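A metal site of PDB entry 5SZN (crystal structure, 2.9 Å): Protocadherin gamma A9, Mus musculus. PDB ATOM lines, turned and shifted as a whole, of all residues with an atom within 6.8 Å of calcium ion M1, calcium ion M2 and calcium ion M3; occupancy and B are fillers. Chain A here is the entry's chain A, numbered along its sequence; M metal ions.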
ATOM      1  N   GLU A 225      14.522   7.092 -31.728  1.00  0.00           N
ATOM      2  CA  GLU A 225      15.758   7.384 -31.021  1.00  0.00           C
ATOM      3  C   GLU A 225      16.742   6.219 -31.058  1.00  0.00           C
ATOM      4  O   GLU A 225      17.957   6.436 -30.960  1.00  0.00           O
ATOM      5  CB  GLU A 225      15.456   7.765 -29.561  1.00  0.00           C
ATOM      6  CG  GLU A 225      14.585   6.767 -28.812  1.00  0.00           C
ATOM      7  CD  GLU A 225      14.365   7.153 -27.365  1.00  0.00           C
ATOM      8  OE1 GLU A 225      15.177   7.925 -26.825  1.00  0.00           O
ATOM      9  OE2 GLU A 225      13.366   6.688 -26.766  1.00  0.00           O
ATOM     10  N   ASN A 226      16.250   4.990 -31.218  1.00  0.00           N
ATOM     11  CA  ASN A 226      17.100   3.814 -31.255  1.00  0.00           C
ATOM     12  C   ASN A 226      17.834   3.699 -32.579  1.00  0.00           C
ATOM     13  O   ASN A 226      18.302   2.614 -32.956  1.00  0.00           O
ATOM     14  CB  ASN A 226      16.269   2.560 -30.998  1.00  0.00           C
ATOM     15  CG  ASN A 226      15.071   2.455 -31.936  1.00  0.00           C
ATOM     16  OD1 ASN A 226      15.018   3.119 -32.967  1.00  0.00           O
ATOM     17  ND2 ASN A 226      14.124   1.604 -31.574  1.00  0.00           N
ATOM     18  N   LEU A 279      21.170   8.754 -30.828  1.00  0.00           N
ATOM     19  CA  LEU A 279      20.266   9.815 -30.414  1.00  0.00           C
ATOM     20  C   LEU A 279      19.476   9.394 -29.175  1.00  0.00           C
ATOM     21  O   LEU A 279      19.450   8.233 -28.783  1.00  0.00           O
ATOM     22  CB  LEU A 279      19.317  10.197 -31.545  1.00  0.00           C
ATOM     23  CG  LEU A 279      19.966  10.820 -32.780  1.00  0.00           C
ATOM     24  CD1 LEU A 279      18.922  11.181 -33.822  1.00  0.00           C
ATOM     25  CD2 LEU A 279      20.786  12.051 -32.387  1.00  0.00           C
ATOM     26  N   ASP A 280      18.818  10.382 -28.575  1.00  0.00           N
ATOM     27  CA  ASP A 280      18.046  10.151 -27.348  1.00  0.00           C
ATOM     28  C   ASP A 280      16.887  11.134 -27.310  1.00  0.00           C
ATOM     29  O   ASP A 280      17.095  12.349 -27.288  1.00  0.00           O
ATOM     30  CB  ASP A 280      18.930  10.319 -26.118  1.00  0.00           C
ATOM     31  CG  ASP A 280      18.312   9.709 -24.878  1.00  0.00           C
ATOM     32  OD1 ASP A 280      17.615   8.688 -25.000  1.00  0.00           O
ATOM     33  OD2 ASP A 280      18.536  10.257 -23.777  1.00  0.00           O
ATOM     34  N   TYR A 281      15.656  10.598 -27.302  1.00  0.00           N
ATOM     35  CA  TYR A 281      14.471  11.449 -27.260  1.00  0.00           C
ATOM     36  C   TYR A 281      14.441  12.317 -26.013  1.00  0.00           C
ATOM     37  O   TYR A 281      13.931  13.444 -26.060  1.00  0.00           O
ATOM     38  CB  TYR A 281      13.213  10.582 -27.337  1.00  0.00           C
ATOM     39  CG  TYR A 281      11.903  11.359 -27.345  1.00  0.00           C
ATOM     40  CD1 TYR A 281      11.336  11.774 -28.545  1.00  0.00           C
ATOM     41  CD2 TYR A 281      11.239  11.654 -26.170  1.00  0.00           C
ATOM     42  CE1 TYR A 281      10.148  12.483 -28.565  1.00  0.00           C
ATOM     43  CE2 TYR A 281      10.048  12.350 -26.179  1.00  0.00           C
ATOM     44  CZ  TYR A 281       9.508  12.758 -27.378  1.00  0.00           C
ATOM     45  OH  TYR A 281       8.326  13.464 -27.391  1.00  0.00           O
ATOM     46  N   GLU A 282      14.978  11.827 -24.907  1.00  0.00           N
ATOM     47  CA  GLU A 282      14.934  12.581 -23.658  1.00  0.00           C
ATOM     48  C   GLU A 282      15.959  13.709 -23.636  1.00  0.00           C
ATOM     49  O   GLU A 282      15.736  14.729 -22.983  1.00  0.00           O
ATOM     50  CB  GLU A 282      15.156  11.646 -22.464  1.00  0.00           C
ATOM     51  CG  GLU A 282      14.043  10.630 -22.257  1.00  0.00           C
ATOM     52  CD  GLU A 282      14.091   9.480 -23.239  1.00  0.00           C
ATOM     53  OE1 GLU A 282      15.145   9.274 -23.872  1.00  0.00           O
ATOM     54  OE2 GLU A 282      13.071   8.774 -23.383  1.00  0.00           O
ATOM     55  N   GLU A 310      11.359  10.486 -32.154  1.00  0.00           N
ATOM     56  CA  GLU A 310      10.204  10.024 -31.415  1.00  0.00           C
ATOM     57  C   GLU A 310      10.648   9.026 -30.347  1.00  0.00           C
ATOM     58  O   GLU A 310      11.667   8.348 -30.502  1.00  0.00           O
ATOM     59  CB  GLU A 310       9.153   9.392 -32.331  1.00  0.00           C
ATOM     60  CG  GLU A 310       8.583  10.356 -33.359  1.00  0.00           C
ATOM     61  CD  GLU A 310       7.784  11.486 -32.724  1.00  0.00           C
ATOM     62  OE1 GLU A 310       6.691  11.222 -32.204  1.00  0.00           O
ATOM     63  OE2 GLU A 310       8.269  12.637 -32.751  1.00  0.00           O
ATOM     64  N   ASP A 311       9.872   8.940 -29.276  1.00  0.00           N
ATOM     65  CA  ASP A 311      10.274   8.170 -28.108  1.00  0.00           C
ATOM     66  C   ASP A 311      10.171   6.672 -28.368  1.00  0.00           C
ATOM     67  O   ASP A 311       9.355   6.211 -29.173  1.00  0.00           O
ATOM     68  CB  ASP A 311       9.423   8.565 -26.904  1.00  0.00           C
ATOM     69  CG  ASP A 311       9.792   7.792 -25.652  1.00  0.00           C
ATOM     70  OD1 ASP A 311      10.904   8.000 -25.127  1.00  0.00           O
ATOM     71  OD2 ASP A 311       8.959   6.975 -25.193  1.00  0.00           O
ATOM     72  N   VAL A 312      11.019   5.907 -27.677  1.00  0.00           N
ATOM     73  CA  VAL A 312      11.031   4.455 -27.763  1.00  0.00           C
ATOM     74  C   VAL A 312      11.157   3.900 -26.351  1.00  0.00           C
ATOM     75  O   VAL A 312      11.853   4.474 -25.502  1.00  0.00           O
ATOM     76  CB  VAL A 312      12.177   3.935 -28.664  1.00  0.00           C
ATOM     77  CG1 VAL A 312      12.243   2.416 -28.660  1.00  0.00           C
ATOM     78  CG2 VAL A 312      11.995   4.440 -30.079  1.00  0.00           C
ATOM     79  N   ASN A 313      10.462   2.790 -26.078  1.00  0.00           N
ATOM     80  CA  ASN A 313      10.558   2.125 -24.788  1.00  0.00           C
ATOM     81  C   ASN A 313      11.936   1.502 -24.571  1.00  0.00           C
ATOM     82  O   ASN A 313      12.122   0.320 -24.843  1.00  0.00           O
ATOM     83  CB  ASN A 313       9.471   1.059 -24.657  1.00  0.00           C
ATOM     84  CG  ASN A 313       9.321   0.536 -23.239  1.00  0.00           C
ATOM     85  OD1 ASN A 313       9.735   1.193 -22.286  1.00  0.00           O
ATOM     86  ND2 ASN A 313       8.723  -0.638 -23.097  1.00  0.00           N
ATOM     87  N   ASP A 314      12.902   2.297 -24.099  1.00  0.00           N
ATOM     88  CA  ASP A 314      14.240   1.826 -23.778  1.00  0.00           C
ATOM     89  C   ASP A 314      14.635   2.191 -22.362  1.00  0.00           C
ATOM     90  O   ASP A 314      15.822   2.351 -22.054  1.00  0.00           O
ATOM     91  CB  ASP A 314      15.267   2.354 -24.782  1.00  0.00           C
ATOM     92  CG  ASP A 314      15.436   3.860 -24.703  1.00  0.00           C
ATOM     93  OD1 ASP A 314      14.451   4.550 -24.375  1.00  0.00           O
ATOM     94  OD2 ASP A 314      16.551   4.364 -24.977  1.00  0.00           O
ATOM     95  N   ASN A 315      13.651   2.361 -21.484  1.00  0.00           N
ATOM     96  CA  ASN A 315      13.882   2.706 -20.088  1.00  0.00           C
ATOM     97  C   ASN A 315      12.938   1.905 -19.212  1.00  0.00           C
ATOM     98  O   ASN A 315      11.839   1.529 -19.628  1.00  0.00           O
ATOM     99  CB  ASN A 315      13.687   4.204 -19.846  1.00  0.00           C
ATOM    100  CG  ASN A 315      14.724   5.055 -20.542  1.00  0.00           C
ATOM    101  OD1 ASN A 315      15.792   5.320 -19.994  1.00  0.00           O
ATOM    102  ND2 ASN A 315      14.426   5.466 -21.770  1.00  0.00           N
ATOM    103  N   ARG A 316      13.387   1.640 -17.952  1.00  0.00           N
ATOM    104  CA  ARG A 316      12.679   0.867 -16.947  1.00  0.00           C
ATOM    105  C   ARG A 316      12.033   1.785 -15.910  1.00  0.00           C
ATOM    106  O   ARG A 316      12.526   2.881 -15.643  1.00  0.00           O
ATOM    107  CB  ARG A 316      13.631  -0.096 -16.241  1.00  0.00           C
ATOM    108  CG  ARG A 316      13.818  -1.419 -16.960  1.00  0.00           C
ATOM    109  CD  ARG A 316      14.659  -2.369 -16.122  1.00  0.00           C
ATOM    110  NE  ARG A 316      14.644  -3.721 -16.662  1.00  0.00           N
ATOM    111  CZ  ARG A 316      15.471  -4.155 -17.607  1.00  0.00           C
ATOM    112  NH1 ARG A 316      16.371  -3.338 -18.126  1.00  0.00           N
ATOM    113  NH2 ARG A 316      15.381  -5.411 -18.036  1.00  0.00           N
ATOM    114  N   PRO A 317      10.919   1.350 -15.322  1.00  0.00           N
ATOM    115  CA  PRO A 317      10.280   2.148 -14.276  1.00  0.00           C
ATOM    116  C   PRO A 317      11.182   2.272 -13.053  1.00  0.00           C
ATOM    117  O   PRO A 317      11.983   1.385 -12.759  1.00  0.00           O
ATOM    118  CB  PRO A 317       9.003   1.375 -13.954  1.00  0.00           C
ATOM    119  CG  PRO A 317       8.759   0.520 -15.164  1.00  0.00           C
ATOM    120  CD  PRO A 317      10.117   0.170 -15.679  1.00  0.00           C
ATOM    121  N   ASP A 345       8.397   6.669 -14.707  1.00  0.00           N
ATOM    122  CA  ASP A 345       9.123   6.212 -15.886  1.00  0.00           C
ATOM    123  C   ASP A 345       9.689   7.420 -16.635  1.00  0.00           C
ATOM    124  O   ASP A 345       9.078   8.491 -16.660  1.00  0.00           O
ATOM    125  CB  ASP A 345       8.230   5.388 -16.817  1.00  0.00           C
ATOM    126  CG  ASP A 345       9.021   4.563 -17.812  1.00  0.00           C
ATOM    127  OD1 ASP A 345      10.050   5.043 -18.332  1.00  0.00           O
ATOM    128  OD2 ASP A 345       8.602   3.409 -18.086  1.00  0.00           O
ATOM    129  N   GLN A 346      10.870   7.228 -17.232  1.00  0.00           N
ATOM    130  CA  GLN A 346      11.484   8.302 -18.000  1.00  0.00           C
ATOM    131  C   GLN A 346      10.833   8.472 -19.366  1.00  0.00           C
ATOM    132  O   GLN A 346      10.820   9.573 -19.906  1.00  0.00           O
ATOM    133  CB  GLN A 346      12.981   8.025 -18.181  1.00  0.00           C
ATOM    134  CG  GLN A 346      13.730   7.804 -16.870  1.00  0.00           C
ATOM    135  CD  GLN A 346      15.202   7.512 -17.092  1.00  0.00           C
ATOM    136  OE1 GLN A 346      15.688   7.535 -18.231  1.00  0.00           O
ATOM    137  NE2 GLN A 346      15.918   7.240 -16.014  1.00  0.00           N
ATOM    138  N   ASP A 347      10.275   7.399 -19.917  1.00  0.00           N
ATOM    139  CA  ASP A 347       9.652   7.454 -21.234  1.00  0.00           C
ATOM    140  C   ASP A 347       8.351   8.247 -21.186  1.00  0.00           C
ATOM    141  O   ASP A 347       7.857   8.625 -20.123  1.00  0.00           O
ATOM    142  CB  ASP A 347       9.405   6.048 -21.762  1.00  0.00           C
ATOM    143  CG  ASP A 347      10.688   5.278 -22.010  1.00  0.00           C
ATOM    144  OD1 ASP A 347      11.684   5.901 -22.434  1.00  0.00           O
ATOM    145  OD2 ASP A 347      10.700   4.044 -21.784  1.00  0.00           O
ATOM    146  N   SER A 348       7.790   8.485 -22.360  1.00  0.00           N
ATOM    147  CA  SER A 348       6.554   9.249 -22.511  1.00  0.00           C
ATOM    148  C   SER A 348       5.465   8.351 -23.090  1.00  0.00           C
ATOM    149  O   SER A 348       5.732   7.285 -23.648  1.00  0.00           O
ATOM    150  CB  SER A 348       6.770  10.462 -23.414  1.00  0.00           C
ATOM    151  OG  SER A 348       7.860  11.255 -22.967  1.00  0.00           O
ATOM    152  N   LYS A 350       2.426   5.788 -23.715  1.00  0.00           N
ATOM    153  CA  LYS A 350       2.200   4.415 -23.258  1.00  0.00           C
ATOM    154  C   LYS A 350       3.474   3.764 -22.751  1.00  0.00           C
ATOM    155  O   LYS A 350       3.393   2.780 -22.002  1.00  0.00           O
ATOM    156  CB  LYS A 350       1.603   3.584 -24.399  1.00  0.00           C
ATOM    157  N   ASN A 351       4.643   4.264 -23.145  1.00  0.00           N
ATOM    158  CA  ASN A 351       5.901   3.793 -22.583  1.00  0.00           C
ATOM    159  C   ASN A 351       6.209   4.393 -21.222  1.00  0.00           C
ATOM    160  O   ASN A 351       7.138   3.930 -20.549  1.00  0.00           O
ATOM    161  CB  ASN A 351       7.047   4.095 -23.556  1.00  0.00           C
ATOM    162  CG  ASN A 351       6.846   3.484 -24.931  1.00  0.00           C
ATOM    163  OD1 ASN A 351       6.388   2.342 -25.053  1.00  0.00           O
ATOM    164  ND2 ASN A 351       7.186   4.237 -25.973  1.00  0.00           N
ATOM    165  N   GLY A 352       5.462   5.415 -20.797  1.00  0.00           N
ATOM    166  CA  GLY A 352       5.699   6.067 -19.533  1.00  0.00           C
ATOM    167  C   GLY A 352       4.690   5.709 -18.466  1.00  0.00           C
ATOM    168  O   GLY A 352       4.922   5.916 -17.276  1.00  0.00           O
ATOM    169  N   GLN A 353       3.536   5.166 -18.882  1.00  0.00           N
ATOM    170  CA  GLN A 353       2.537   4.717 -17.922  1.00  0.00           C
ATOM    171  C   GLN A 353       3.034   3.475 -17.197  1.00  0.00           C
ATOM    172  O   GLN A 353       3.625   2.567 -17.799  1.00  0.00           O
ATOM    173  CB  GLN A 353       1.213   4.423 -18.623  1.00  0.00           C
ATOM    174  CG  GLN A 353       0.577   5.645 -19.264  1.00  0.00           C
ATOM    175  CD  GLN A 353      -0.751   5.310 -19.923  1.00  0.00           C
ATOM    176  OE1 GLN A 353      -1.284   4.223 -19.769  1.00  0.00           O
ATOM    177  NE2 GLN A 353      -1.282   6.261 -20.682  1.00  0.00           N
ATOM    178  N   ASP A 398       5.756  -1.361 -17.187  1.00  0.00           N
ATOM    179  CA  ASP A 398       5.217  -0.270 -17.987  1.00  0.00           C
ATOM    180  C   ASP A 398       4.200  -0.804 -18.986  1.00  0.00           C
ATOM    181  O   ASP A 398       4.126  -2.008 -19.263  1.00  0.00           O
ATOM    182  CB  ASP A 398       6.326   0.513 -18.692  1.00  0.00           C
ATOM    183  CG  ASP A 398       7.192  -0.351 -19.603  1.00  0.00           C
ATOM    184  OD1 ASP A 398       6.796  -1.481 -19.957  1.00  0.00           O
ATOM    185  OD2 ASP A 398       8.294   0.118 -19.981  1.00  0.00           O
ATOM    186  N   ARG A 399       3.406   0.106 -19.545  1.00  0.00           N
ATOM    187  CA  ARG A 399       2.328  -0.247 -20.449  1.00  0.00           C
ATOM    188  C   ARG A 399       2.747  -0.209 -21.919  1.00  0.00           C
ATOM    189  O   ARG A 399       1.893  -0.389 -22.800  1.00  0.00           O
ATOM    190  CB  ARG A 399       1.126   0.677 -20.217  1.00  0.00           C
ATOM    191  CG  ARG A 399      -0.226   0.003 -20.433  1.00  0.00           C
ATOM    192  CD  ARG A 399      -1.362   1.005 -20.279  1.00  0.00           C
ATOM    193  NE  ARG A 399      -1.474   1.526 -18.923  1.00  0.00           N
ATOM    194  CZ  ARG A 399      -2.269   1.014 -17.989  1.00  0.00           C
ATOM    195  NH1 ARG A 399      -3.016  -0.054 -18.258  1.00  0.00           N
ATOM    196  NH2 ARG A 399      -2.312   1.556 -16.783  1.00  0.00           N
ATOM    197  N   GLY A 400       4.032   0.004 -22.208  1.00  0.00           N
ATOM    198  CA  GLY A 400       4.505   0.066 -23.573  1.00  0.00           C
ATOM    199  C   GLY A 400       4.787  -1.300 -24.169  1.00  0.00           C
ATOM    200  O   GLY A 400       4.541  -2.347 -23.559  1.00  0.00           O
ATOM    201  N   MET A 404       8.693  -3.366 -20.131  1.00  0.00           N
ATOM    202  CA  MET A 404       9.836  -3.460 -19.237  1.00  0.00           C
ATOM    203  C   MET A 404       9.358  -3.358 -17.806  1.00  0.00           C
ATOM    204  O   MET A 404       8.661  -2.406 -17.443  1.00  0.00           O
ATOM    205  CB  MET A 404      10.864  -2.360 -19.527  1.00  0.00           C
ATOM    206  CG  MET A 404      11.574  -2.488 -20.863  1.00  0.00           C
ATOM    207  SD  MET A 404      12.931  -1.302 -21.009  1.00  0.00           S
ATOM    208  CE  MET A 404      13.609  -1.770 -22.602  1.00  0.00           C
HETATM  209 CA    CA M   1      16.379   6.703 -24.736  1.00  0.00          CA
HETATM  210 CA    CA M   2      13.143   6.583 -24.414  1.00  0.00          CA
HETATM  211 CA    CA M   3       9.503   2.888 -20.225  1.00  0.00          CA
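Within 4 Å of calcium ion M1: Glu 225, Asp 280, Glu 282, Asp 314 and Asn 315. The nearest printed residue that does not touch calcium ion M1 is Tyr 281 (4.7 Å).
The backbone NH (N) of Glu 225 is in hydrogen-bond range of the backbone carbonyl oxygen (O) of Glu 310, 3.4 Å away. OE1 of Glu 225 lies close to N of Tyr 281 (2.8 Å). The side-chain carboxylate of Asp 311 lies within hydrogen-bond range of the side-chain amide nitrogen of Asn 351 (3.4 Å). The backbone NH (N) of Ser 348 sits at hydrogen-bond distance from the side-chain carboxylate (OD2) of Asp 311 (3.4 Å). The side-chain amide oxygen (OE1) of Gln 346 sits close to the side-chain amide oxygen (OD1) of Asn 315 (2.8 Å). N of Asn 315 sits close to SD of Met 404 (3.8 Å). The side-chain carboxylate (OD1) of Asp 398 lies within hydrogen-bond range of the backbone NH (N) of Met 404 (2.7 Å). ND2 of Asn 313 is in hydrogen-bond range of OD2 of Asp 398 (3.2 Å).
Of the 26 residues printed, 7 come within 4 Å of calcium ion M2.
Calcium ion M3 is bound by OD2 of Asp 347 (2.3 Å), OD2 of Asp 345 (2.4 Å), O of Asn 351 (2.6 Å), OD1 of Asn 313 (2.7 Å) and O of Asn 315 (2.8 Å). Slightly farther from calcium ion M3 lies the side-chain carboxylate (OD1) of Asp 345 (2.9 Å). Slightly farther from calcium ion M3 lies OD2 of Asp 398 (3.0 Å).
Calcium ion M2 is bound by OE2 of Glu 225 (2.4 Å), OD1 of Asp 314 (2.4 Å), OE2 of Glu 282 (2.4 Å), OD1 of Asp 347 (2.6 Å), O of Val 312 (2.7 Å) and OD1 of Asp 311 (2.7 Å). Slightly farther from calcium ion M2 lies ND2 of Asn 315 (3.1 Å).
Six residues have an atom within 4 Å of calcium ion M3: Asn 313, Asn 315, Asp 345, Asp 347, Asn 351 and Asp 398. The nearest printed residue that does not touch calcium ion M3 is Arg 316 (4.7 Å).
Calcium ion M1 is bound by the side-chain carboxylate of Asp 280 (2.4 Å), the side-chain carboxylate of Asp 314 (2.4 Å) and the side-chain carboxylate of Glu 225 (2.7 Å). Slightly farther from calcium ion M1 lies the side-chain carboxylate (OD1) of Asp 314 (2.9 Å). Slightly farther from calcium ion M1 lies OE1 of Glu 282 (3.0 Å).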
